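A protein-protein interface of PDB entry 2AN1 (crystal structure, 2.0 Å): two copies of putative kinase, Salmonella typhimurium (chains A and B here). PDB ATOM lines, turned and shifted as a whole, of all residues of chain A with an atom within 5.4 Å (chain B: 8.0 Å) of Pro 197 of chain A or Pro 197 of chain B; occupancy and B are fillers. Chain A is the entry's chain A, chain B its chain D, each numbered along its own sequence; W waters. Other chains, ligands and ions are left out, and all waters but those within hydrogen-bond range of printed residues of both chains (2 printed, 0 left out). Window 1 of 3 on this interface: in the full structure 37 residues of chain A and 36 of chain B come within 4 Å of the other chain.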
ATOM      1  N   SER A 187      23.908   8.978  15.796  1.00  0.00           N
ATOM      2  CA  SER A 187      23.315   9.918  14.823  1.00  0.00           C
ATOM      3  C   SER A 187      23.593   9.519  13.376  1.00  0.00           C
ATOM      4  O   SER A 187      22.922   9.972  12.451  1.00  0.00           O
ATOM      5  CB  SER A 187      23.793  11.350  15.092  1.00  0.00           C
ATOM      6  OG  SER A 187      25.122  11.533  14.631  1.00  0.00           O
ATOM      7  N   SER A 191      18.900   6.744  13.542  1.00  0.00           N
ATOM      8  CA  SER A 191      18.499   8.153  13.481  1.00  0.00           C
ATOM      9  C   SER A 191      18.676   8.778  12.081  1.00  0.00           C
ATOM     10  O   SER A 191      17.809   9.516  11.611  1.00  0.00           O
ATOM     11  CB  SER A 191      19.281   8.967  14.512  1.00  0.00           C
ATOM     12  OG  SER A 191      18.713  10.257  14.615  1.00  0.00           O
ATOM     13  N   LEU A 192      19.782   8.451  11.420  1.00  0.00           N
ATOM     14  CA  LEU A 192      20.091   9.007  10.085  1.00  0.00           C
ATOM     15  C   LEU A 192      19.115   8.531   9.005  1.00  0.00           C
ATOM     16  O   LEU A 192      18.653   9.323   8.183  1.00  0.00           O
ATOM     17  CB  LEU A 192      21.521   8.651   9.668  1.00  0.00           C
ATOM     18  CG  LEU A 192      22.085   9.483   8.504  1.00  0.00           C
ATOM     19  CD1 LEU A 192      22.188  10.949   8.927  1.00  0.00           C
ATOM     20  CD2 LEU A 192      23.431   8.933   8.095  1.00  0.00           C
ATOM     21  N   GLY A 195      15.928  10.370   9.029  1.00  0.00           N
ATOM     22  CA  GLY A 195      15.956  11.782   8.654  1.00  0.00           C
ATOM     23  C   GLY A 195      16.605  12.726   9.660  1.00  0.00           C
ATOM     24  O   GLY A 195      16.499  13.967   9.522  1.00  0.00           O
ATOM     25  N   GLY A 196      17.274  12.175  10.672  1.00  0.00           N
ATOM     26  CA  GLY A 196      17.871  13.027  11.716  1.00  0.00           C
ATOM     27  C   GLY A 196      19.149  13.703  11.244  1.00  0.00           C
ATOM     28  O   GLY A 196      19.695  13.332  10.217  1.00  0.00           O
ATOM     29  N   PRO A 197      19.648  14.698  12.005  1.00  0.00           N
ATOM     30  CA  PRO A 197      20.923  15.302  11.627  1.00  0.00           C
ATOM     31  C   PRO A 197      22.112  14.466  12.111  1.00  0.00           C
ATOM     32  O   PRO A 197      21.962  13.622  13.014  1.00  0.00           O
ATOM     33  CB  PRO A 197      20.905  16.641  12.373  1.00  0.00           C
ATOM     34  CG  PRO A 197      20.184  16.334  13.625  1.00  0.00           C
ATOM     35  CD  PRO A 197      19.090  15.322  13.217  1.00  0.00           C
ATOM     36  N   ILE A 198      23.271  14.739  11.523  1.00  0.00           N
ATOM     37  CA  ILE A 198      24.536  14.167  11.941  1.00  0.00           C
ATOM     38  C   ILE A 198      25.129  15.076  13.027  1.00  0.00           C
ATOM     39  O   ILE A 198      25.223  16.293  12.848  1.00  0.00           O
ATOM     40  CB  ILE A 198      25.522  14.077  10.756  1.00  0.00           C
ATOM     41  CG1 ILE A 198      24.947  13.172   9.672  1.00  0.00           C
ATOM     42  CG2 ILE A 198      26.894  13.502  11.199  1.00  0.00           C
ATOM     43  CD1 ILE A 198      25.457  13.480   8.294  1.00  0.00           C
ATOM     44  N   LEU A 199      25.534  14.461  14.134  1.00  0.00           N
ATOM     45  CA  LEU A 199      26.149  15.161  15.252  1.00  0.00           C
ATOM     46  C   LEU A 199      27.599  14.703  15.365  1.00  0.00           C
ATOM     47  O   LEU A 199      27.849  13.506  15.458  1.00  0.00           O
ATOM     48  CB  LEU A 199      25.409  14.801  16.548  1.00  0.00           C
ATOM     49  CG  LEU A 199      24.188  15.612  17.019  1.00  0.00           C
ATOM     50  CD1 LEU A 199      23.115  15.801  15.970  1.00  0.00           C
ATOM     51  CD2 LEU A 199      23.604  15.020  18.335  1.00  0.00           C
ATOM     52  N   THR A 207      19.682  13.899  20.251  1.00  0.00           N
ATOM     53  CA  THR A 207      18.674  14.268  19.268  1.00  0.00           C
ATOM     54  C   THR A 207      17.439  13.424  19.436  1.00  0.00           C
ATOM     55  O   THR A 207      17.538  12.229  19.676  1.00  0.00           O
ATOM     56  CB  THR A 207      19.189  14.105  17.812  1.00  0.00           C
ATOM     57  OG1 THR A 207      20.490  14.678  17.713  1.00  0.00           O
ATOM     58  CG2 THR A 207      18.271  14.828  16.841  1.00  0.00           C
ATOM     59  N   VAL A 209      14.252  12.285  17.353  1.00  0.00           N
ATOM     60  CA  VAL A 209      13.852  12.189  15.942  1.00  0.00           C
ATOM     61  C   VAL A 209      12.519  11.447  15.871  1.00  0.00           C
ATOM     62  O   VAL A 209      12.439  10.279  16.265  1.00  0.00           O
ATOM     63  CB  VAL A 209      14.948  11.503  15.081  1.00  0.00           C
ATOM     64  CG1 VAL A 209      14.450  11.262  13.629  1.00  0.00           C
ATOM     65  CG2 VAL A 209      16.202  12.350  15.064  1.00  0.00           C
ATOM     66  N   PRO A 220      13.396  17.175  13.800  1.00  0.00           N
ATOM     67  CA  PRO A 220      14.391  16.718  14.751  1.00  0.00           C
ATOM     68  C   PRO A 220      14.782  17.860  15.687  1.00  0.00           C
ATOM     69  O   PRO A 220      14.894  19.024  15.260  1.00  0.00           O
ATOM     70  CB  PRO A 220      15.580  16.360  13.862  1.00  0.00           C
ATOM     71  CG  PRO A 220      14.953  15.973  12.545  1.00  0.00           C
ATOM     72  CD  PRO A 220      13.861  16.993  12.405  1.00  0.00           C
ATOM     73  N   LEU A 221      14.963  17.514  16.953  1.00  0.00           N
ATOM     74  CA  LEU A 221      15.272  18.490  17.982  1.00  0.00           C
ATOM     75  C   LEU A 221      16.572  18.086  18.661  1.00  0.00           C
ATOM     76  O   LEU A 221      16.757  16.918  18.993  1.00  0.00           O
ATOM     77  CB  LEU A 221      14.120  18.529  18.990  1.00  0.00           C
ATOM     78  CG  LEU A 221      14.251  19.294  20.305  1.00  0.00           C
ATOM     79  CD1 LEU A 221      14.565  20.784  20.126  1.00  0.00           C
ATOM     80  CD2 LEU A 221      12.946  19.096  21.072  1.00  0.00           C
ATOM     81  N   VAL A 222      17.486  19.034  18.852  1.00  0.00           N
ATOM     82  CA  VAL A 222      18.762  18.695  19.455  1.00  0.00           C
ATOM     83  C   VAL A 222      18.870  19.425  20.791  1.00  0.00           C
ATOM     84  O   VAL A 222      18.757  20.657  20.844  1.00  0.00           O
ATOM     85  CB  VAL A 222      19.952  19.070  18.547  1.00  0.00           C
ATOM     86  CG1 VAL A 222      21.246  18.595  19.179  1.00  0.00           C
ATOM     87  CG2 VAL A 222      19.783  18.490  17.115  1.00  0.00           C
ATOM     88  N   SER B 182      24.132  28.166  11.095  1.00  0.00           N
ATOM     89  CA  SER B 182      23.163  28.764  11.990  1.00  0.00           C
ATOM     90  C   SER B 182      23.525  28.533  13.462  1.00  0.00           C
ATOM     91  O   SER B 182      24.057  27.472  13.819  1.00  0.00           O
ATOM     92  CB  SER B 182      21.787  28.160  11.686  1.00  0.00           C
ATOM     93  OG  SER B 182      20.834  28.550  12.672  1.00  0.00           O
ATOM     94  N   THR B 183      23.228  29.524  14.309  1.00  0.00           N
ATOM     95  CA  THR B 183      23.284  29.369  15.760  1.00  0.00           C
ATOM     96  C   THR B 183      22.001  28.634  16.189  1.00  0.00           C
ATOM     97  O   THR B 183      21.121  28.441  15.357  1.00  0.00           O
ATOM     98  CB  THR B 183      23.269  30.727  16.446  1.00  0.00           C
ATOM     99  OG1 THR B 183      22.043  31.392  16.107  1.00  0.00           O
ATOM    100  CG2 THR B 183      24.459  31.585  16.002  1.00  0.00           C
ATOM    101  N   PRO B 184      21.898  28.210  17.472  1.00  0.00           N
ATOM    102  CA  PRO B 184      20.619  27.755  18.032  1.00  0.00           C
ATOM    103  C   PRO B 184      19.472  28.762  17.867  1.00  0.00           C
ATOM    104  O   PRO B 184      18.354  28.352  17.572  1.00  0.00           O
ATOM    105  CB  PRO B 184      20.953  27.538  19.514  1.00  0.00           C
ATOM    106  CG  PRO B 184      22.358  27.094  19.471  1.00  0.00           C
ATOM    107  CD  PRO B 184      22.976  28.059  18.472  1.00  0.00           C
ATOM    108  N   GLY B 186      19.210  30.971  15.422  1.00  0.00           N
ATOM    109  CA  GLY B 186      18.831  30.909  14.022  1.00  0.00           C
ATOM    110  C   GLY B 186      18.188  29.617  13.564  1.00  0.00           C
ATOM    111  O   GLY B 186      17.686  29.564  12.441  1.00  0.00           O
ATOM    112  N   SER B 187      18.219  28.569  14.399  1.00  0.00           N
ATOM    113  CA  SER B 187      17.797  27.213  13.951  1.00  0.00           C
ATOM    114  C   SER B 187      16.304  27.097  13.691  1.00  0.00           C
ATOM    115  O   SER B 187      15.854  26.162  13.040  1.00  0.00           O
ATOM    116  CB  SER B 187      18.253  26.114  14.926  1.00  0.00           C
ATOM    117  OG  SER B 187      17.582  26.203  16.180  1.00  0.00           O
ATOM    118  N   THR B 188      15.532  28.061  14.187  1.00  0.00           N
ATOM    119  CA  THR B 188      14.086  28.043  13.995  1.00  0.00           C
ATOM    120  C   THR B 188      13.682  29.023  12.876  1.00  0.00           C
ATOM    121  O   THR B 188      12.493  29.176  12.577  1.00  0.00           O
ATOM    122  CB  THR B 188      13.332  28.410  15.302  1.00  0.00           C
ATOM    123  OG1 THR B 188      13.839  29.649  15.798  1.00  0.00           O
ATOM    124  CG2 THR B 188      13.515  27.322  16.378  1.00  0.00           C
ATOM    125  N   ALA B 189      14.675  29.654  12.256  1.00  0.00           N
ATOM    126  CA  ALA B 189      14.443  30.685  11.232  1.00  0.00           C
ATOM    127  C   ALA B 189      14.702  30.097   9.844  1.00  0.00           C
ATOM    128  O   ALA B 189      14.202  29.012   9.529  1.00  0.00           O
ATOM    129  CB  ALA B 189      15.350  31.896  11.507  1.00  0.00           C
ATOM    130  N   SER B 191      17.198  28.515   8.516  1.00  0.00           N
ATOM    131  CA  SER B 191      17.727  27.163   8.657  1.00  0.00           C
ATOM    132  C   SER B 191      16.589  26.128   8.733  1.00  0.00           C
ATOM    133  O   SER B 191      16.662  25.056   8.130  1.00  0.00           O
ATOM    134  CB  SER B 191      18.570  27.105   9.935  1.00  0.00           C
ATOM    135  OG  SER B 191      19.187  25.845  10.071  1.00  0.00           O
ATOM    136  N   LEU B 192      15.539  26.469   9.471  1.00  0.00           N
ATOM    137  CA  LEU B 192      14.440  25.534   9.676  1.00  0.00           C
ATOM    138  C   LEU B 192      13.688  25.364   8.360  1.00  0.00           C
ATOM    139  O   LEU B 192      13.360  24.255   8.006  1.00  0.00           O
ATOM    140  CB  LEU B 192      13.513  25.997  10.794  1.00  0.00           C
ATOM    141  CG  LEU B 192      12.470  24.975  11.285  1.00  0.00           C
ATOM    142  CD1 LEU B 192      13.168  23.838  12.016  1.00  0.00           C
ATOM    143  CD2 LEU B 192      11.426  25.669  12.173  1.00  0.00           C
ATOM    144  N   ALA B 194      14.945  25.531   5.487  1.00  0.00           N
ATOM    145  CA  ALA B 194      15.810  24.740   4.602  1.00  0.00           C
ATOM    146  C   ALA B 194      15.996  23.286   5.039  1.00  0.00           C
ATOM    147  O   ALA B 194      16.839  22.587   4.484  1.00  0.00           O
ATOM    148  CB  ALA B 194      17.198  25.440   4.417  1.00  0.00           C
ATOM    149  N   GLY B 195      15.258  22.847   6.057  1.00  0.00           N
ATOM    150  CA  GLY B 195      15.321  21.463   6.536  1.00  0.00           C
ATOM    151  C   GLY B 195      16.292  21.172   7.664  1.00  0.00           C
ATOM    152  O   GLY B 195      16.591  20.011   7.943  1.00  0.00           O
ATOM    153  N   GLY B 196      16.778  22.215   8.329  1.00  0.00           N
ATOM    154  CA  GLY B 196      17.719  22.031   9.434  1.00  0.00           C
ATOM    155  C   GLY B 196      17.027  21.534  10.701  1.00  0.00           C
ATOM    156  O   GLY B 196      15.795  21.612  10.809  1.00  0.00           O
ATOM    157  N   PRO B 197      17.814  21.050  11.686  1.00  0.00           N
ATOM    158  CA  PRO B 197      17.201  20.652  12.961  1.00  0.00           C
ATOM    159  C   PRO B 197      17.018  21.852  13.881  1.00  0.00           C
ATOM    160  O   PRO B 197      17.718  22.865  13.731  1.00  0.00           O
ATOM    161  CB  PRO B 197      18.245  19.698  13.562  1.00  0.00           C
ATOM    162  CG  PRO B 197      19.568  20.272  13.075  1.00  0.00           C
ATOM    163  CD  PRO B 197      19.285  20.854  11.686  1.00  0.00           C
ATOM    164  N   ILE B 198      16.125  21.716  14.856  1.00  0.00           N
ATOM    165  CA  ILE B 198      15.979  22.709  15.940  1.00  0.00           C
ATOM    166  C   ILE B 198      17.033  22.454  17.028  1.00  0.00           C
ATOM    167  O   ILE B 198      17.155  21.326  17.501  1.00  0.00           O
ATOM    168  CB  ILE B 198      14.587  22.615  16.574  1.00  0.00           C
ATOM    169  CG1 ILE B 198      13.505  22.770  15.494  1.00  0.00           C
ATOM    170  CG2 ILE B 198      14.425  23.644  17.740  1.00  0.00           C
ATOM    171  CD1 ILE B 198      12.269  21.998  15.799  1.00  0.00           C
ATOM    172  N   LEU B 199      17.796  23.488  17.391  1.00  0.00           N
ATOM    173  CA  LEU B 199      18.758  23.421  18.491  1.00  0.00           C
ATOM    174  C   LEU B 199      18.250  24.267  19.655  1.00  0.00           C
ATOM    175  O   LEU B 199      17.867  25.423  19.467  1.00  0.00           O
ATOM    176  CB  LEU B 199      20.116  23.962  18.075  1.00  0.00           C
ATOM    177  CG  LEU B 199      21.122  23.082  17.329  1.00  0.00           C
ATOM    178  CD1 LEU B 199      20.480  22.160  16.301  1.00  0.00           C
ATOM    179  CD2 LEU B 199      22.153  23.998  16.682  1.00  0.00           C
ATOM    180  N   THR B 200      18.285  23.699  20.858  1.00  0.00           N
ATOM    181  CA  THR B 200      17.801  24.414  22.032  1.00  0.00           C
ATOM    182  C   THR B 200      18.723  25.621  22.251  1.00  0.00           C
ATOM    183  O   THR B 200      19.939  25.518  22.031  1.00  0.00           O
ATOM    184  CB  THR B 200      17.760  23.503  23.270  1.00  0.00           C
ATOM    185  OG1 THR B 200      19.041  22.891  23.438  1.00  0.00           O
ATOM    186  CG2 THR B 200      16.698  22.415  23.089  1.00  0.00           C
ATOM    187  N   ILE B 206      26.642  24.575  16.534  1.00  0.00           N
ATOM    188  CA  ILE B 206      26.417  25.320  15.302  1.00  0.00           C
ATOM    189  C   ILE B 206      25.962  24.263  14.301  1.00  0.00           C
ATOM    190  O   ILE B 206      26.484  23.138  14.308  1.00  0.00           O
ATOM    191  CB  ILE B 206      27.753  25.947  14.802  1.00  0.00           C
ATOM    192  CG1 ILE B 206      28.194  27.117  15.700  1.00  0.00           C
ATOM    193  CG2 ILE B 206      27.651  26.415  13.338  1.00  0.00           C
ATOM    194  CD1 ILE B 206      29.736  27.453  15.565  1.00  0.00           C
ATOM    195  N   THR B 207      24.989  24.602  13.450  1.00  0.00           N
ATOM    196  CA  THR B 207      24.530  23.669  12.420  1.00  0.00           C
ATOM    197  C   THR B 207      24.865  24.167  11.025  1.00  0.00           C
ATOM    198  O   THR B 207      24.722  25.347  10.733  1.00  0.00           O
ATOM    199  CB  THR B 207      23.016  23.390  12.525  1.00  0.00           C
ATOM    200  OG1 THR B 207      22.717  23.122  13.893  1.00  0.00           O
ATOM    201  CG2 THR B 207      22.640  22.150  11.713  1.00  0.00           C
ATOM    202  N   LEU B 208      25.322  23.246  10.182  1.00  0.00           N
ATOM    203  CA  LEU B 208      25.622  23.523   8.773  1.00  0.00           C
ATOM    204  C   LEU B 208      24.543  22.827   7.957  1.00  0.00           C
ATOM    205  O   LEU B 208      24.395  21.600   8.030  1.00  0.00           O
ATOM    206  CB  LEU B 208      27.004  22.975   8.387  1.00  0.00           C
ATOM    207  CG  LEU B 208      28.231  23.644   9.036  1.00  0.00           C
ATOM    208  CD1 LEU B 208      28.384  23.183  10.482  1.00  0.00           C
ATOM    209  CD2 LEU B 208      29.489  23.316   8.257  1.00  0.00           C
ATOM    210  N   VAL B 209      23.783  23.617   7.202  1.00  0.00           N
ATOM    211  CA  VAL B 209      22.593  23.137   6.495  1.00  0.00           C
ATOM    212  C   VAL B 209      22.762  23.416   4.997  1.00  0.00           C
ATOM    213  O   VAL B 209      22.825  24.572   4.594  1.00  0.00           O
ATOM    214  CB  VAL B 209      21.311  23.825   7.077  1.00  0.00           C
ATOM    215  CG1 VAL B 209      20.051  23.485   6.268  1.00  0.00           C
ATOM    216  CG2 VAL B 209      21.137  23.474   8.576  1.00  0.00           C
ATOM    217  N   ARG B 219      23.321  15.806   4.476  1.00  0.00           N
ATOM    218  CA  ARG B 219      22.390  15.958   5.607  1.00  0.00           C
ATOM    219  C   ARG B 219      22.917  17.083   6.475  1.00  0.00           C
ATOM    220  O   ARG B 219      24.125  17.306   6.491  1.00  0.00           O
ATOM    221  CB  ARG B 219      22.296  14.670   6.442  1.00  0.00           C
ATOM    222  CG  ARG B 219      21.566  13.474   5.783  1.00  0.00           C
ATOM    223  CD  ARG B 219      20.057  13.711   5.542  1.00  0.00           C
ATOM    224  NE  ARG B 219      19.409  12.555   4.881  1.00  0.00           N
ATOM    225  CZ  ARG B 219      19.466  12.268   3.571  1.00  0.00           C
ATOM    226  NH1 ARG B 219      20.179  13.021   2.708  1.00  0.00           N
ATOM    227  NH2 ARG B 219      18.809  11.202   3.106  1.00  0.00           N
ATOM    228  N   PRO B 220      22.034  17.794   7.197  1.00  0.00           N
ATOM    229  CA  PRO B 220      22.562  18.787   8.142  1.00  0.00           C
ATOM    230  C   PRO B 220      23.566  18.177   9.136  1.00  0.00           C
ATOM    231  O   PRO B 220      23.422  17.022   9.565  1.00  0.00           O
ATOM    232  CB  PRO B 220      21.315  19.249   8.892  1.00  0.00           C
ATOM    233  CG  PRO B 220      20.202  19.016   7.909  1.00  0.00           C
ATOM    234  CD  PRO B 220      20.558  17.742   7.222  1.00  0.00           C
ATOM    235  N   LEU B 221      24.578  18.964   9.463  1.00  0.00           N
ATOM    236  CA  LEU B 221      25.638  18.562  10.342  1.00  0.00           C
ATOM    237  C   LEU B 221      25.641  19.540  11.522  1.00  0.00           C
ATOM    238  O   LEU B 221      25.489  20.753  11.326  1.00  0.00           O
ATOM    239  CB  LEU B 221      26.970  18.624   9.575  1.00  0.00           C
ATOM    240  CG  LEU B 221      28.262  18.357  10.358  1.00  0.00           C
ATOM    241  CD1 LEU B 221      28.364  16.902  10.754  1.00  0.00           C
ATOM    242  CD2 LEU B 221      29.464  18.766   9.506  1.00  0.00           C
ATOM    243  N   VAL B 222      25.799  19.008  12.731  1.00  0.00           N
ATOM    244  CA  VAL B 222      25.808  19.806  13.944  1.00  0.00           C
ATOM    245  C   VAL B 222      27.167  19.614  14.574  1.00  0.00           C
ATOM    246  O   VAL B 222      27.561  18.478  14.856  1.00  0.00           O
ATOM    247  CB  VAL B 222      24.710  19.357  14.935  1.00  0.00           C
ATOM    248  CG1 VAL B 222      24.698  20.257  16.167  1.00  0.00           C
ATOM    249  CG2 VAL B 222      23.334  19.396  14.250  1.00  0.00           C
HETATM  250  O   HOH W   1      17.516  10.288   5.851  1.00  0.00           O
HETATM  251  O   HOH W   2      19.068  11.945   7.751  1.00  0.00           O
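The backbone carbonyl oxygen (O) of Pro 220 of chain B lies within hydrogen-bond range of the backbone NH (N) of Ile 198 of chain A, 3.0 Å away.
O of Pro 220 of chain A sits at hydrogen-bond distance from N of Ile 198 of chain B (3.0 Å).
O of Val 222 of chain A lies within hydrogen-bond range of N of Thr 200 of chain B.
The backbone carbonyl oxygen of Ile 198 of chain B lies within hydrogen-bond range of the backbone NH of Val 222 of chain A.
The backbone NH of Val 222 of chain B lies within hydrogen-bond range of the backbone carbonyl oxygen of Ile 198 of chain A, 2.8 Å away.
The backbone NH of Leu 208 of chain B is in hydrogen-bond range of the backbone carbonyl oxygen of Leu 221 of chain B (2.7 Å).
The side-chain hydroxyl (OG) of Ser 187 of chain A is in hydrogen-bond range of the backbone NH (N) of Leu 199 of chain A (3.0 Å).
N of Leu 199 of chain B is in hydrogen-bond range of OG of Ser 187 of chain B (3.0 Å).
Among the printed residues, pairs that only touch across the chains: Ile 198 of chain A with Leu 221 of chain B (3.4 Å), Leu 221 of chain A with Ile 198 of chain B (3.4 Å), Leu 199 of chain A with Val 222 of chain B (3.6 Å), Val 222 of chain A with Leu 199 of chain B (3.6 Å), Pro 220 of chain A with Pro 197 of chain B (3.6 Å), Pro 197 of chain A with Pro 220 of chain B (3.7 Å), Ile 198 of chain A with Arg 219 of chain B (3.9 Å), Pro 197 of chain A with Pro 197 of chain B (3.9 Å) and Leu 221 of chain A with Thr 200 of chain B (3.999 Å).
Pro 197 of chain B touches just these residues of chain A: Pro 197 (3.9 Å) and Pro 220 (3.6 Å).
No residue of chain B comes within 4 Å of Gly 196 of chain A.
Of the printed residues of chain B, Val 222 of chain A touches Ile 198, Leu 199 and Thr 200.
Of the printed residues of chain B, Leu 199 of chain A touches Val 222 (3.6 Å).
Printed residues of chain B within 4 Å of Pro 220 of chain A: Pro 197 and Ile 198.
Of the printed residues of chain B, Leu 221 of chain A touches Ile 198 (3.4 Å) and Thr 200 (3.999 Å).
Printed residues of chain A within 4 Å of Val 222 of chain B: Ile 198 and Leu 199.
Leu 192 of chain B touches none of the printed residues of chain A.
The nearest residue of chain A that does not touch Pro 197 of chain B is Val 222 of chain A (4.1 Å).
Hydrophobic or aromatic side chains of chain A within 4 Å of the printed part of chain B: Pro 197, Ile 198, Leu 199, Leu 221 and Val 222.
Among the printed residues, no Asp or Glu carboxylate lies within 4 Å of a Lys or Arg side-chain nitrogen of the other chain.
Pro 197 of chain A touches Pro 220 of chain B, and with the chains exchanged Pro 220 of chain A touches Pro 197 of chain B.
Ile 198 of chain A touches Leu 221 of chain B, and with the chains exchanged Leu 221 of chain A touches Ile 198 of chain B.
Ile 198 of chain A touches Val 222 of chain B, and with the chains exchanged Val 222 of chain A touches Ile 198 of chain B.
Leu 199 of chain A touches Val 222 of chain B, and with the chains exchanged Val 222 of chain A touches Leu 199 of chain B.
13 positions are printed for both chains.
Water W2 lies within hydrogen-bond range of the backbone carbonyl oxygen (O) of Leu 192 of chain A (2.7 Å), the backbone carbonyl oxygen (O) of Gly 196 of chain A (2.9 Å) and the guanidinium group (NE) of Arg 219 of chain B (3.0 Å).
Water W1 lies within hydrogen-bond range of O of Leu 192 of chain A (2.8 Å) and NE of Arg 219 of chain B (3.1 Å).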
